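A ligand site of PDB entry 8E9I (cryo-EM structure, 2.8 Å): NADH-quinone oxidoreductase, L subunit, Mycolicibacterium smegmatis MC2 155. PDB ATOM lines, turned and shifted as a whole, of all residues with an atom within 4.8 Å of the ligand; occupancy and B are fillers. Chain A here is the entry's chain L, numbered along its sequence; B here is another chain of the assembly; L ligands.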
ATOM      1  N   PRO A 166      -8.310  13.281  -0.544  1.00  0.00           N
ATOM      2  CA  PRO A 166      -7.968  12.095   0.264  1.00  0.00           C
ATOM      3  C   PRO A 166      -9.173  11.446   0.891  1.00  0.00           C
ATOM      4  O   PRO A 166      -9.179  10.218   1.101  1.00  0.00           O
ATOM      5  CB  PRO A 166      -7.006  12.671   1.318  1.00  0.00           C
ATOM      6  CG  PRO A 166      -6.501  13.934   0.745  1.00  0.00           C
ATOM      7  CD  PRO A 166      -7.632  14.490  -0.047  1.00  0.00           C
ATOM      8  N   SER A 167     -10.201  12.227   1.219  1.00  0.00           N
ATOM      9  CA  SER A 167     -11.419  11.651   1.773  1.00  0.00           C
ATOM     10  C   SER A 167     -12.075  10.705   0.780  1.00  0.00           C
ATOM     11  O   SER A 167     -12.580   9.642   1.153  1.00  0.00           O
ATOM     12  CB  SER A 167     -12.394  12.753   2.168  1.00  0.00           C
ATOM     13  OG  SER A 167     -12.819  13.481   1.024  1.00  0.00           O
ATOM     14  N   THR A 170     -10.068   7.439   0.784  1.00  0.00           N
ATOM     15  CA  THR A 170     -10.260   6.673   2.009  1.00  0.00           C
ATOM     16  C   THR A 170     -11.655   6.048   2.038  1.00  0.00           C
ATOM     17  O   THR A 170     -11.808   4.882   2.433  1.00  0.00           O
ATOM     18  CB  THR A 170     -10.055   7.574   3.221  1.00  0.00           C
ATOM     19  OG1 THR A 170      -8.729   8.137   3.169  1.00  0.00           O
ATOM     20  CG2 THR A 170     -10.219   6.794   4.512  1.00  0.00           C
ATOM     21  N   LYS A 174     -12.389   2.041   2.252  1.00  0.00           N
ATOM     22  CA  LYS A 174     -13.173   1.449   3.336  1.00  0.00           C
ATOM     23  C   LYS A 174     -14.385   0.715   2.803  1.00  0.00           C
ATOM     24  O   LYS A 174     -14.696  -0.408   3.226  1.00  0.00           O
ATOM     25  CB  LYS A 174     -13.593   2.530   4.327  1.00  0.00           C
ATOM     26  N   VAL A 177     -13.286  -2.538   1.150  1.00  0.00           N
ATOM     27  CA  VAL A 177     -12.770  -3.543   2.076  1.00  0.00           C
ATOM     28  C   VAL A 177     -13.915  -4.167   2.874  1.00  0.00           C
ATOM     29  O   VAL A 177     -13.933  -5.376   3.120  1.00  0.00           O
ATOM     30  CB  VAL A 177     -11.709  -2.928   3.001  1.00  0.00           C
ATOM     31  CG1 VAL A 177     -11.312  -3.929   4.077  1.00  0.00           C
ATOM     32  CG2 VAL A 177     -10.490  -2.508   2.190  1.00  0.00           C
ATOM     33  N   VAL A 178     -14.880  -3.350   3.302  1.00  0.00           N
ATOM     34  CA  VAL A 178     -16.052  -3.917   3.964  1.00  0.00           C
ATOM     35  C   VAL A 178     -16.830  -4.792   3.004  1.00  0.00           C
ATOM     36  O   VAL A 178     -17.280  -5.900   3.351  1.00  0.00           O
ATOM     37  CB  VAL A 178     -16.919  -2.797   4.549  1.00  0.00           C
ATOM     38  CG1 VAL A 178     -18.189  -3.362   5.138  1.00  0.00           C
ATOM     39  CG2 VAL A 178     -16.151  -2.041   5.616  1.00  0.00           C
ATOM     40  N   VAL A 181     -15.097  -8.014   2.917  1.00  0.00           N
ATOM     41  CA  VAL A 181     -15.487  -8.873   4.028  1.00  0.00           C
ATOM     42  C   VAL A 181     -16.779  -9.597   3.688  1.00  0.00           C
ATOM     43  O   VAL A 181     -16.920 -10.808   3.887  1.00  0.00           O
ATOM     44  CB  VAL A 181     -15.643  -8.050   5.315  1.00  0.00           C
ATOM     45  CG1 VAL A 181     -16.239  -8.907   6.420  1.00  0.00           C
ATOM     46  CG2 VAL A 181     -14.298  -7.489   5.740  1.00  0.00           C
ATOM     47  N   LEU A 226     -24.433 -12.251   5.851  1.00  0.00           N
ATOM     48  CA  LEU A 226     -23.231 -11.446   6.041  1.00  0.00           C
ATOM     49  C   LEU A 226     -22.841 -10.739   4.758  1.00  0.00           C
ATOM     50  O   LEU A 226     -22.457  -9.564   4.777  1.00  0.00           O
ATOM     51  CB  LEU A 226     -22.084 -12.333   6.528  1.00  0.00           C
ATOM     52  CG  LEU A 226     -20.740 -11.621   6.702  1.00  0.00           C
ATOM     53  CD1 LEU A 226     -20.837 -10.537   7.768  1.00  0.00           C
ATOM     54  CD2 LEU A 226     -19.654 -12.611   7.066  1.00  0.00           C
ATOM     55  N   PRO A 236     -22.343  -5.749  11.207  1.00  0.00           N
ATOM     56  CA  PRO A 236     -21.435  -4.721  11.718  1.00  0.00           C
ATOM     57  C   PRO A 236     -20.698  -3.969  10.605  1.00  0.00           C
ATOM     58  O   PRO A 236     -19.841  -3.122  10.871  1.00  0.00           O
ATOM     59  CB  PRO A 236     -20.456  -5.512  12.582  1.00  0.00           C
ATOM     60  N   ASP A 553     -17.651   3.595  13.384  1.00  0.00           N
ATOM     61  CA  ASP A 553     -16.335   3.659  12.759  1.00  0.00           C
ATOM     62  C   ASP A 553     -15.233   3.369  13.777  1.00  0.00           C
ATOM     63  O   ASP A 553     -14.335   2.569  13.525  1.00  0.00           O
ATOM     64  CB  ASP A 553     -16.120   5.029  12.123  1.00  0.00           C
ATOM     65  N   ALA A 554     -15.315   4.008  14.950  1.00  0.00           N
ATOM     66  CA  ALA A 554     -14.315   3.746  15.980  1.00  0.00           C
ATOM     67  C   ALA A 554     -14.257   2.265  16.329  1.00  0.00           C
ATOM     68  O   ALA A 554     -13.174   1.715  16.543  1.00  0.00           O
ATOM     69  CB  ALA A 554     -14.617   4.571  17.228  1.00  0.00           C
ATOM     70  N   ASN A 556     -14.596  -0.176  14.407  1.00  0.00           N
ATOM     71  CA  ASN A 556     -13.670  -0.727  13.429  1.00  0.00           C
ATOM     72  C   ASN A 556     -12.254  -0.227  13.684  1.00  0.00           C
ATOM     73  O   ASN A 556     -11.296  -1.007  13.687  1.00  0.00           O
ATOM     74  CB  ASN A 556     -14.115  -0.359  12.017  1.00  0.00           C
ATOM     75  CG  ASN A 556     -15.425  -1.008  11.623  1.00  0.00           C
ATOM     76  OD1 ASN A 556     -16.263  -0.397  10.961  1.00  0.00           O
ATOM     77  ND2 ASN A 556     -15.607  -2.264  12.014  1.00  0.00           N
ATOM     78  N   GLU A 557     -12.104   1.080  13.907  1.00  0.00           N
ATOM     79  CA  GLU A 557     -10.772   1.650  14.084  1.00  0.00           C
ATOM     80  C   GLU A 557     -10.111   1.107  15.348  1.00  0.00           C
ATOM     81  O   GLU A 557      -8.889   0.918  15.381  1.00  0.00           O
ATOM     82  CB  GLU A 557     -10.873   3.179  14.141  1.00  0.00           C
ATOM     83  N   PHE A 560     -10.391  -3.501  15.013  1.00  0.00           N
ATOM     84  CA  PHE A 560      -9.756  -4.035  13.812  1.00  0.00           C
ATOM     85  C   PHE A 560      -8.523  -3.260  13.384  1.00  0.00           C
ATOM     86  O   PHE A 560      -7.425  -3.821  13.329  1.00  0.00           O
ATOM     87  CB  PHE A 560     -10.772  -4.062  12.668  1.00  0.00           C
ATOM     88  CG  PHE A 560     -11.858  -5.083  12.846  1.00  0.00           C
ATOM     89  CD1 PHE A 560     -12.982  -4.790  13.589  1.00  0.00           C
ATOM     90  CD2 PHE A 560     -11.744  -6.335  12.274  1.00  0.00           C
ATOM     91  CE1 PHE A 560     -13.980  -5.732  13.746  1.00  0.00           C
ATOM     92  CE2 PHE A 560     -12.731  -7.285  12.431  1.00  0.00           C
ATOM     93  CZ  PHE A 560     -13.845  -6.978  13.170  1.00  0.00           C
ATOM     94  N   MET A 561      -8.658  -1.967  13.073  1.00  0.00           N
ATOM     95  CA  MET A 561      -7.524  -1.216  12.553  1.00  0.00           C
ATOM     96  C   MET A 561      -6.364  -1.257  13.529  1.00  0.00           C
ATOM     97  O   MET A 561      -5.240  -1.599  13.156  1.00  0.00           O
ATOM     98  CB  MET A 561      -7.925   0.236  12.267  1.00  0.00           C
ATOM     99  CG  MET A 561      -6.803   1.109  11.723  1.00  0.00           C
ATOM    100  SD  MET A 561      -6.819   2.767  12.432  1.00  0.00           S
ATOM    101  CE  MET A 561      -5.950   2.493  13.970  1.00  0.00           C
ATOM    102  N   GLY A 564      -5.369  -4.872  13.796  1.00  0.00           N
ATOM    103  CA  GLY A 564      -4.715  -5.251  12.555  1.00  0.00           C
ATOM    104  C   GLY A 564      -3.294  -4.723  12.477  1.00  0.00           C
ATOM    105  O   GLY A 564      -2.385  -5.421  12.036  1.00  0.00           O
ATOM    106  N   GLN A 565      -3.092  -3.477  12.904  1.00  0.00           N
ATOM    107  CA  GLN A 565      -1.742  -2.922  12.929  1.00  0.00           C
ATOM    108  C   GLN A 565      -0.876  -3.674  13.935  1.00  0.00           C
ATOM    109  O   GLN A 565       0.314  -3.892  13.693  1.00  0.00           O
ATOM    110  CB  GLN A 565      -1.801  -1.438  13.269  1.00  0.00           C
ATOM    111  CG  GLN A 565      -2.358  -0.567  12.160  1.00  0.00           C
ATOM    112  CD  GLN A 565      -2.677   0.831  12.635  1.00  0.00           C
ATOM    113  OE1 GLN A 565      -2.517   1.147  13.808  1.00  0.00           O
ATOM    114  NE2 GLN A 565      -3.155   1.666  11.733  1.00  0.00           N
ATOM    115  N   LEU A 567      -1.170  -6.859  14.734  1.00  0.00           N
ATOM    116  CA  LEU A 567      -0.808  -8.109  14.082  1.00  0.00           C
ATOM    117  C   LEU A 567       0.241  -7.880  13.010  1.00  0.00           C
ATOM    118  O   LEU A 567       1.177  -8.682  12.861  1.00  0.00           O
ATOM    119  CB  LEU A 567      -2.058  -8.758  13.485  1.00  0.00           C
ATOM    120  CG  LEU A 567      -1.871 -10.038  12.670  1.00  0.00           C
ATOM    121  CD1 LEU A 567      -1.291 -11.144  13.520  1.00  0.00           C
ATOM    122  CD2 LEU A 567      -3.190 -10.475  12.068  1.00  0.00           C
ATOM    123  N   THR A 568       0.112  -6.799  12.240  1.00  0.00           N
ATOM    124  CA  THR A 568       1.062  -6.503  11.194  1.00  0.00           C
ATOM    125  C   THR A 568       2.455  -6.305  11.759  1.00  0.00           C
ATOM    126  O   THR A 568       3.431  -6.905  11.290  1.00  0.00           O
ATOM    127  CB  THR A 568       0.619  -5.255  10.430  1.00  0.00           C
ATOM    128  OG1 THR A 568      -0.657  -5.492   9.831  1.00  0.00           O
ATOM    129  CG2 THR A 568       1.631  -4.891   9.344  1.00  0.00           C
ATOM    130  N   ILE B 315       1.039  -6.098   3.615  1.00  0.00           N
ATOM    131  CA  ILE B 315       0.377  -4.956   4.236  1.00  0.00           C
ATOM    132  C   ILE B 315       1.389  -4.103   4.975  1.00  0.00           C
ATOM    133  O   ILE B 315       1.376  -2.872   4.882  1.00  0.00           O
ATOM    134  CB  ILE B 315      -0.759  -5.426   5.164  1.00  0.00           C
ATOM    135  CG1 ILE B 315      -1.886  -6.069   4.356  1.00  0.00           C
ATOM    136  CG2 ILE B 315      -1.282  -4.258   5.972  1.00  0.00           C
ATOM    137  CD1 ILE B 315      -2.921  -6.784   5.177  1.00  0.00           C
ATOM    138  N   THR B 436      -9.869 -15.593   4.123  1.00  0.00           N
ATOM    139  CA  THR B 436      -9.537 -14.294   4.712  1.00  0.00           C
ATOM    140  C   THR B 436      -8.559 -13.522   3.836  1.00  0.00           C
ATOM    141  O   THR B 436      -8.526 -12.282   3.851  1.00  0.00           O
ATOM    142  CB  THR B 436      -8.955 -14.488   6.103  1.00  0.00           C
ATOM    143  OG1 THR B 436      -7.731 -15.225   6.012  1.00  0.00           O
ATOM    144  CG2 THR B 436      -9.934 -15.213   6.996  1.00  0.00           C
ATOM    145  N   VAL B 439      -9.890 -10.640   1.818  1.00  0.00           N
ATOM    146  CA  VAL B 439      -9.902  -9.359   2.507  1.00  0.00           C
ATOM    147  C   VAL B 439      -8.500  -8.767   2.554  1.00  0.00           C
ATOM    148  O   VAL B 439      -8.288  -7.574   2.287  1.00  0.00           O
ATOM    149  CB  VAL B 439     -10.492  -9.519   3.918  1.00  0.00           C
ATOM    150  CG1 VAL B 439     -10.478  -8.205   4.655  1.00  0.00           C
ATOM    151  CG2 VAL B 439     -11.902 -10.084   3.846  1.00  0.00           C
ATOM    152  N   LEU B 440      -7.521  -9.589   2.923  1.00  0.00           N
ATOM    153  CA  LEU B 440      -6.159  -9.076   3.097  1.00  0.00           C
ATOM    154  C   LEU B 440      -5.605  -8.526   1.781  1.00  0.00           C
ATOM    155  O   LEU B 440      -4.848  -7.545   1.784  1.00  0.00           O
ATOM    156  CB  LEU B 440      -5.263 -10.167   3.659  1.00  0.00           C
ATOM    157  CG  LEU B 440      -5.732 -10.792   4.965  1.00  0.00           C
ATOM    158  CD1 LEU B 440      -4.886 -11.992   5.328  1.00  0.00           C
ATOM    159  CD2 LEU B 440      -5.718  -9.762   6.077  1.00  0.00           C
ATOM    160  N   VAL B 443      -6.878  -5.196   1.200  1.00  0.00           N
ATOM    161  CA  VAL B 443      -6.142  -4.274   2.050  1.00  0.00           C
ATOM    162  C   VAL B 443      -4.846  -3.837   1.377  1.00  0.00           C
ATOM    163  O   VAL B 443      -4.667  -2.663   1.044  1.00  0.00           O
ATOM    164  CB  VAL B 443      -5.885  -4.888   3.437  1.00  0.00           C
ATOM    165  CG1 VAL B 443      -4.957  -4.009   4.244  1.00  0.00           C
ATOM    166  CG2 VAL B 443      -7.190  -5.078   4.171  1.00  0.00           C
ATOM    167  N   TRP B 447      -4.905  -0.110  -0.326  1.00  0.00           N
ATOM    168  CA  TRP B 447      -4.177   0.850   0.493  1.00  0.00           C
ATOM    169  C   TRP B 447      -2.949   1.366  -0.241  1.00  0.00           C
ATOM    170  O   TRP B 447      -2.639   2.557  -0.188  1.00  0.00           O
ATOM    171  CB  TRP B 447      -3.779   0.223   1.817  1.00  0.00           C
ATOM    172  CG  TRP B 447      -3.298   1.213   2.823  1.00  0.00           C
ATOM    173  CD1 TRP B 447      -3.577   2.546   2.874  1.00  0.00           C
ATOM    174  CD2 TRP B 447      -2.444   0.956   3.944  1.00  0.00           C
ATOM    175  NE1 TRP B 447      -2.961   3.131   3.939  1.00  0.00           N
ATOM    176  CE2 TRP B 447      -2.255   2.168   4.615  1.00  0.00           C
ATOM    177  CE3 TRP B 447      -1.825  -0.195   4.442  1.00  0.00           C
ATOM    178  CZ2 TRP B 447      -1.478   2.272   5.760  1.00  0.00           C
ATOM    179  CZ3 TRP B 447      -1.046  -0.087   5.577  1.00  0.00           C
ATOM    180  CH2 TRP B 447      -0.884   1.136   6.226  1.00  0.00           C
ATOM    181  N   GLN B 450      -4.083   3.752  -2.875  1.00  0.00           N
ATOM    182  CA  GLN B 450      -4.493   4.995  -2.235  1.00  0.00           C
ATOM    183  C   GLN B 450      -3.281   5.840  -1.889  1.00  0.00           C
ATOM    184  O   GLN B 450      -3.224   7.037  -2.207  1.00  0.00           O
ATOM    185  CB  GLN B 450      -5.312   4.677  -0.987  1.00  0.00           C
ATOM    186  CG  GLN B 450      -5.546   5.858  -0.054  1.00  0.00           C
ATOM    187  CD  GLN B 450      -6.400   5.504   1.142  1.00  0.00           C
ATOM    188  OE1 GLN B 450      -6.953   4.415   1.217  1.00  0.00           O
ATOM    189  NE2 GLN B 450      -6.527   6.441   2.076  1.00  0.00           N
HETATM  190  C1  LIG L   1      -7.871   8.557   8.936  1.00  0.00           C
HETATM  191  C2  LIG L   1      -7.720   7.603  10.142  1.00  0.00           C
HETATM  192  C3  LIG L   1      -8.530   6.296   9.984  1.00  0.00           C
HETATM  193  C4  LIG L   1      -8.755   5.990   8.522  1.00  0.00           C
HETATM  194  C5  LIG L   1     -10.094   4.253   9.124  1.00  0.00           C
HETATM  195  C6  LIG L   1     -11.125   2.321  10.234  1.00  0.00           C
HETATM  196  C7  LIG L   1     -11.258   0.818  10.140  1.00  0.00           C
HETATM  197  C8  LIG L   1     -12.338  -0.558   8.443  1.00  0.00           C
HETATM  198  C9  LIG L   1     -12.413  -1.759   9.390  1.00  0.00           C
HETATM  199  C10 LIG L   1     -12.955  -3.003   8.650  1.00  0.00           C
HETATM  200  C11 LIG L   1     -13.622  -4.014   9.580  1.00  0.00           C
HETATM  201  C12 LIG L   1     -14.550  -4.943   8.798  1.00  0.00           C
HETATM  202  C13 LIG L   1     -15.207  -6.013   9.720  1.00  0.00           C
HETATM  203  C14 LIG L   1     -16.321  -5.416  10.591  1.00  0.00           C
HETATM  204  C15 LIG L   1     -17.005  -6.536  11.480  1.00  0.00           C
HETATM  205  C16 LIG L   1     -17.311  -7.818  10.644  1.00  0.00           C
HETATM  206  C17 LIG L   1     -17.978  -8.936  11.504  1.00  0.00           C
HETATM  207  C18 LIG L   1     -18.225 -10.222  10.689  1.00  0.00           C
HETATM  208  C19 LIG L   1     -12.479   2.960   9.890  1.00  0.00           C
HETATM  209  C20 LIG L   1     -12.434   3.669   8.573  1.00  0.00           C
HETATM  210  C21 LIG L   1     -11.411   4.739   8.540  1.00  0.00           C
HETATM  211  C22 LIG L   1      -7.486   6.367   7.781  1.00  0.00           C
HETATM  212  C23 LIG L   1      -6.463   2.222   6.482  1.00  0.00           C
HETATM  213  C24 LIG L   1      -6.571   1.175   7.605  1.00  0.00           C
HETATM  214  C25 LIG L   1      -4.956  -0.508   7.984  1.00  0.00           C
HETATM  215  C26 LIG L   1      -4.643  -2.035   8.033  1.00  0.00           C
HETATM  216  C27 LIG L   1      -3.526  -2.352   9.045  1.00  0.00           C
HETATM  217  C28 LIG L   1      -3.497  -3.887   9.413  1.00  0.00           C
HETATM  218  C29 LIG L   1      -4.824  -4.644   8.979  1.00  0.00           C
HETATM  219  C30 LIG L   1      -4.711  -6.197   9.184  1.00  0.00           C
HETATM  220  C31 LIG L   1      -6.098  -6.886   9.257  1.00  0.00           C
HETATM  221  C32 LIG L   1      -5.999  -8.373   9.655  1.00  0.00           C
HETATM  222  C33 LIG L   1      -8.042   0.979   7.961  1.00  0.00           C
HETATM  223  C34 LIG L   1      -9.049  -1.198   7.787  1.00  0.00           C
HETATM  224  C35 LIG L   1      -8.423  -1.623   9.128  1.00  0.00           C
HETATM  225  C36 LIG L   1      -8.597  -3.146   9.385  1.00  0.00           C
HETATM  226  C37 LIG L   1      -8.051  -3.995   8.176  1.00  0.00           C
HETATM  227  C38 LIG L   1      -8.888  -5.288   7.953  1.00  0.00           C
HETATM  228  C39 LIG L   1     -10.184  -5.262   8.785  1.00  0.00           C
HETATM  229  C40 LIG L   1     -11.036  -6.516   8.562  1.00  0.00           C
HETATM  230  C41 LIG L   1     -10.538  -7.728   9.423  1.00  0.00           C
HETATM  231  C42 LIG L   1     -11.532  -8.911   9.359  1.00  0.00           C
HETATM  232  C43 LIG L   1     -10.796 -10.319   9.134  1.00  0.00           C
HETATM  233  C44 LIG L   1     -11.796 -11.519   9.191  1.00  0.00           C
HETATM  234  C45 LIG L   1      -7.511   7.895   7.615  1.00  0.00           C
HETATM  235  C46 LIG L   1      -6.260   8.416   5.758  1.00  0.00           C
HETATM  236  C47 LIG L   1      -5.011   9.144   5.286  1.00  0.00           C
HETATM  237  C48 LIG L   1      -5.046  10.600   5.631  1.00  0.00           C
HETATM  238  C49 LIG L   1      -6.248  11.223   5.096  1.00  0.00           C
HETATM  239  C50 LIG L   1      -7.488  10.541   5.630  1.00  0.00           C
HETATM  240  C51 LIG L   1      -8.672  11.148   4.985  1.00  0.00           C
HETATM  241  O1  LIG L   1      -7.013   9.658   9.140  1.00  0.00           O
HETATM  242  O2  LIG L   1      -8.182   8.280  11.276  1.00  0.00           O
HETATM  243  O3  LIG L   1      -7.797   5.242  10.559  1.00  0.00           O
HETATM  244  O4  LIG L   1      -9.075   4.571   8.335  1.00  0.00           O
HETATM  245  O5  LIG L   1     -10.087   2.750   9.304  1.00  0.00           O
HETATM  246  O6  LIG L   1     -11.436   0.528   8.725  1.00  0.00           O
HETATM  247  O7  LIG L   1     -13.025  -0.506   7.477  1.00  0.00           O
HETATM  248  O8  LIG L   1     -12.827   3.908  10.914  1.00  0.00           O
HETATM  249  O9  LIG L   1     -12.101   2.688   7.545  1.00  0.00           O
HETATM  250  O10 LIG L   1     -11.227   5.143   7.166  1.00  0.00           O
HETATM  251  O11 LIG L   1      -7.451   5.742   6.495  1.00  0.00           O
HETATM  252  O12 LIG L   1      -6.044   3.472   7.082  1.00  0.00           O
HETATM  253  O13 LIG L   1      -6.038  -0.029   7.164  1.00  0.00           O
HETATM  254  O14 LIG L   1      -4.309   0.250   8.608  1.00  0.00           O
HETATM  255  O15 LIG L   1      -8.550  -0.034   7.081  1.00  0.00           O
HETATM  256  O16 LIG L   1      -9.940  -1.821   7.322  1.00  0.00           O
HETATM  257  O17 LIG L   1      -4.860   5.638   6.362  1.00  0.00           O
HETATM  258  O18 LIG L   1      -6.165   4.421   4.686  1.00  0.00           O
HETATM  259  O19 LIG L   1      -6.243   8.336   7.187  1.00  0.00           O
HETATM  260  O20 LIG L   1      -4.924   9.024   3.884  1.00  0.00           O
HETATM  261  O21 LIG L   1      -3.880  11.241   5.037  1.00  0.00           O
HETATM  262  O22 LIG L   1      -6.267  12.598   5.504  1.00  0.00           O
HETATM  263  O23 LIG L   1      -8.697  10.714   3.625  1.00  0.00           O
HETATM  264  O24 LIG L   1      -7.475   9.075   5.341  1.00  0.00           O
HETATM  265  P1  LIG L   1      -6.093   4.831   6.122  1.00  0.00           P
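An oxygen (O23) of the ligand is in hydrogen-bond range of the side-chain hydroxyl (OG1) of Thr 170 (2.6 Å).
An oxygen (O18) of the ligand is in hydrogen-bond range of the side-chain amide nitrogen of Gln 450 of chain B, 3.3 Å away.
SD of Met 561 sits at hydrogen-bond distance from O3 of the ligand (3.3 Å).
The backbone carbonyl oxygen (O) of Asp 553 sits at hydrogen-bond distance from an oxygen (O8) of the ligand (3.3 Å).
O23 of the ligand lies within hydrogen-bond range of N of Ser 167 (3.2 Å).
The backbone carbonyl oxygen (O) of Pro 166 is in hydrogen-bond range of an oxygen (O23) of the ligand (2.6 Å).
N of Met 561 lies within hydrogen-bond range of O of Asn 556 (2.9 Å).
O of Gly 564 sits at hydrogen-bond distance from OG1 of Thr 568 (2.8 Å).
The side-chain hydroxyl (OG1) of Thr 170 sits at hydrogen-bond distance from the side-chain amide nitrogen (NE2) of Gln 450 of chain B.
O of Pro 166 lies within hydrogen-bond range of OG1 of Thr 170, 3.0 Å away.
Merely in contact with the ligand: Lys 174, Val 178, Val 181, Leu 226, Pro 236, Asn 556, Glu 557, Phe 560, Gly 564, Gln 565, Thr 568, Leu 440 of chain B and Trp 447 of chain B.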
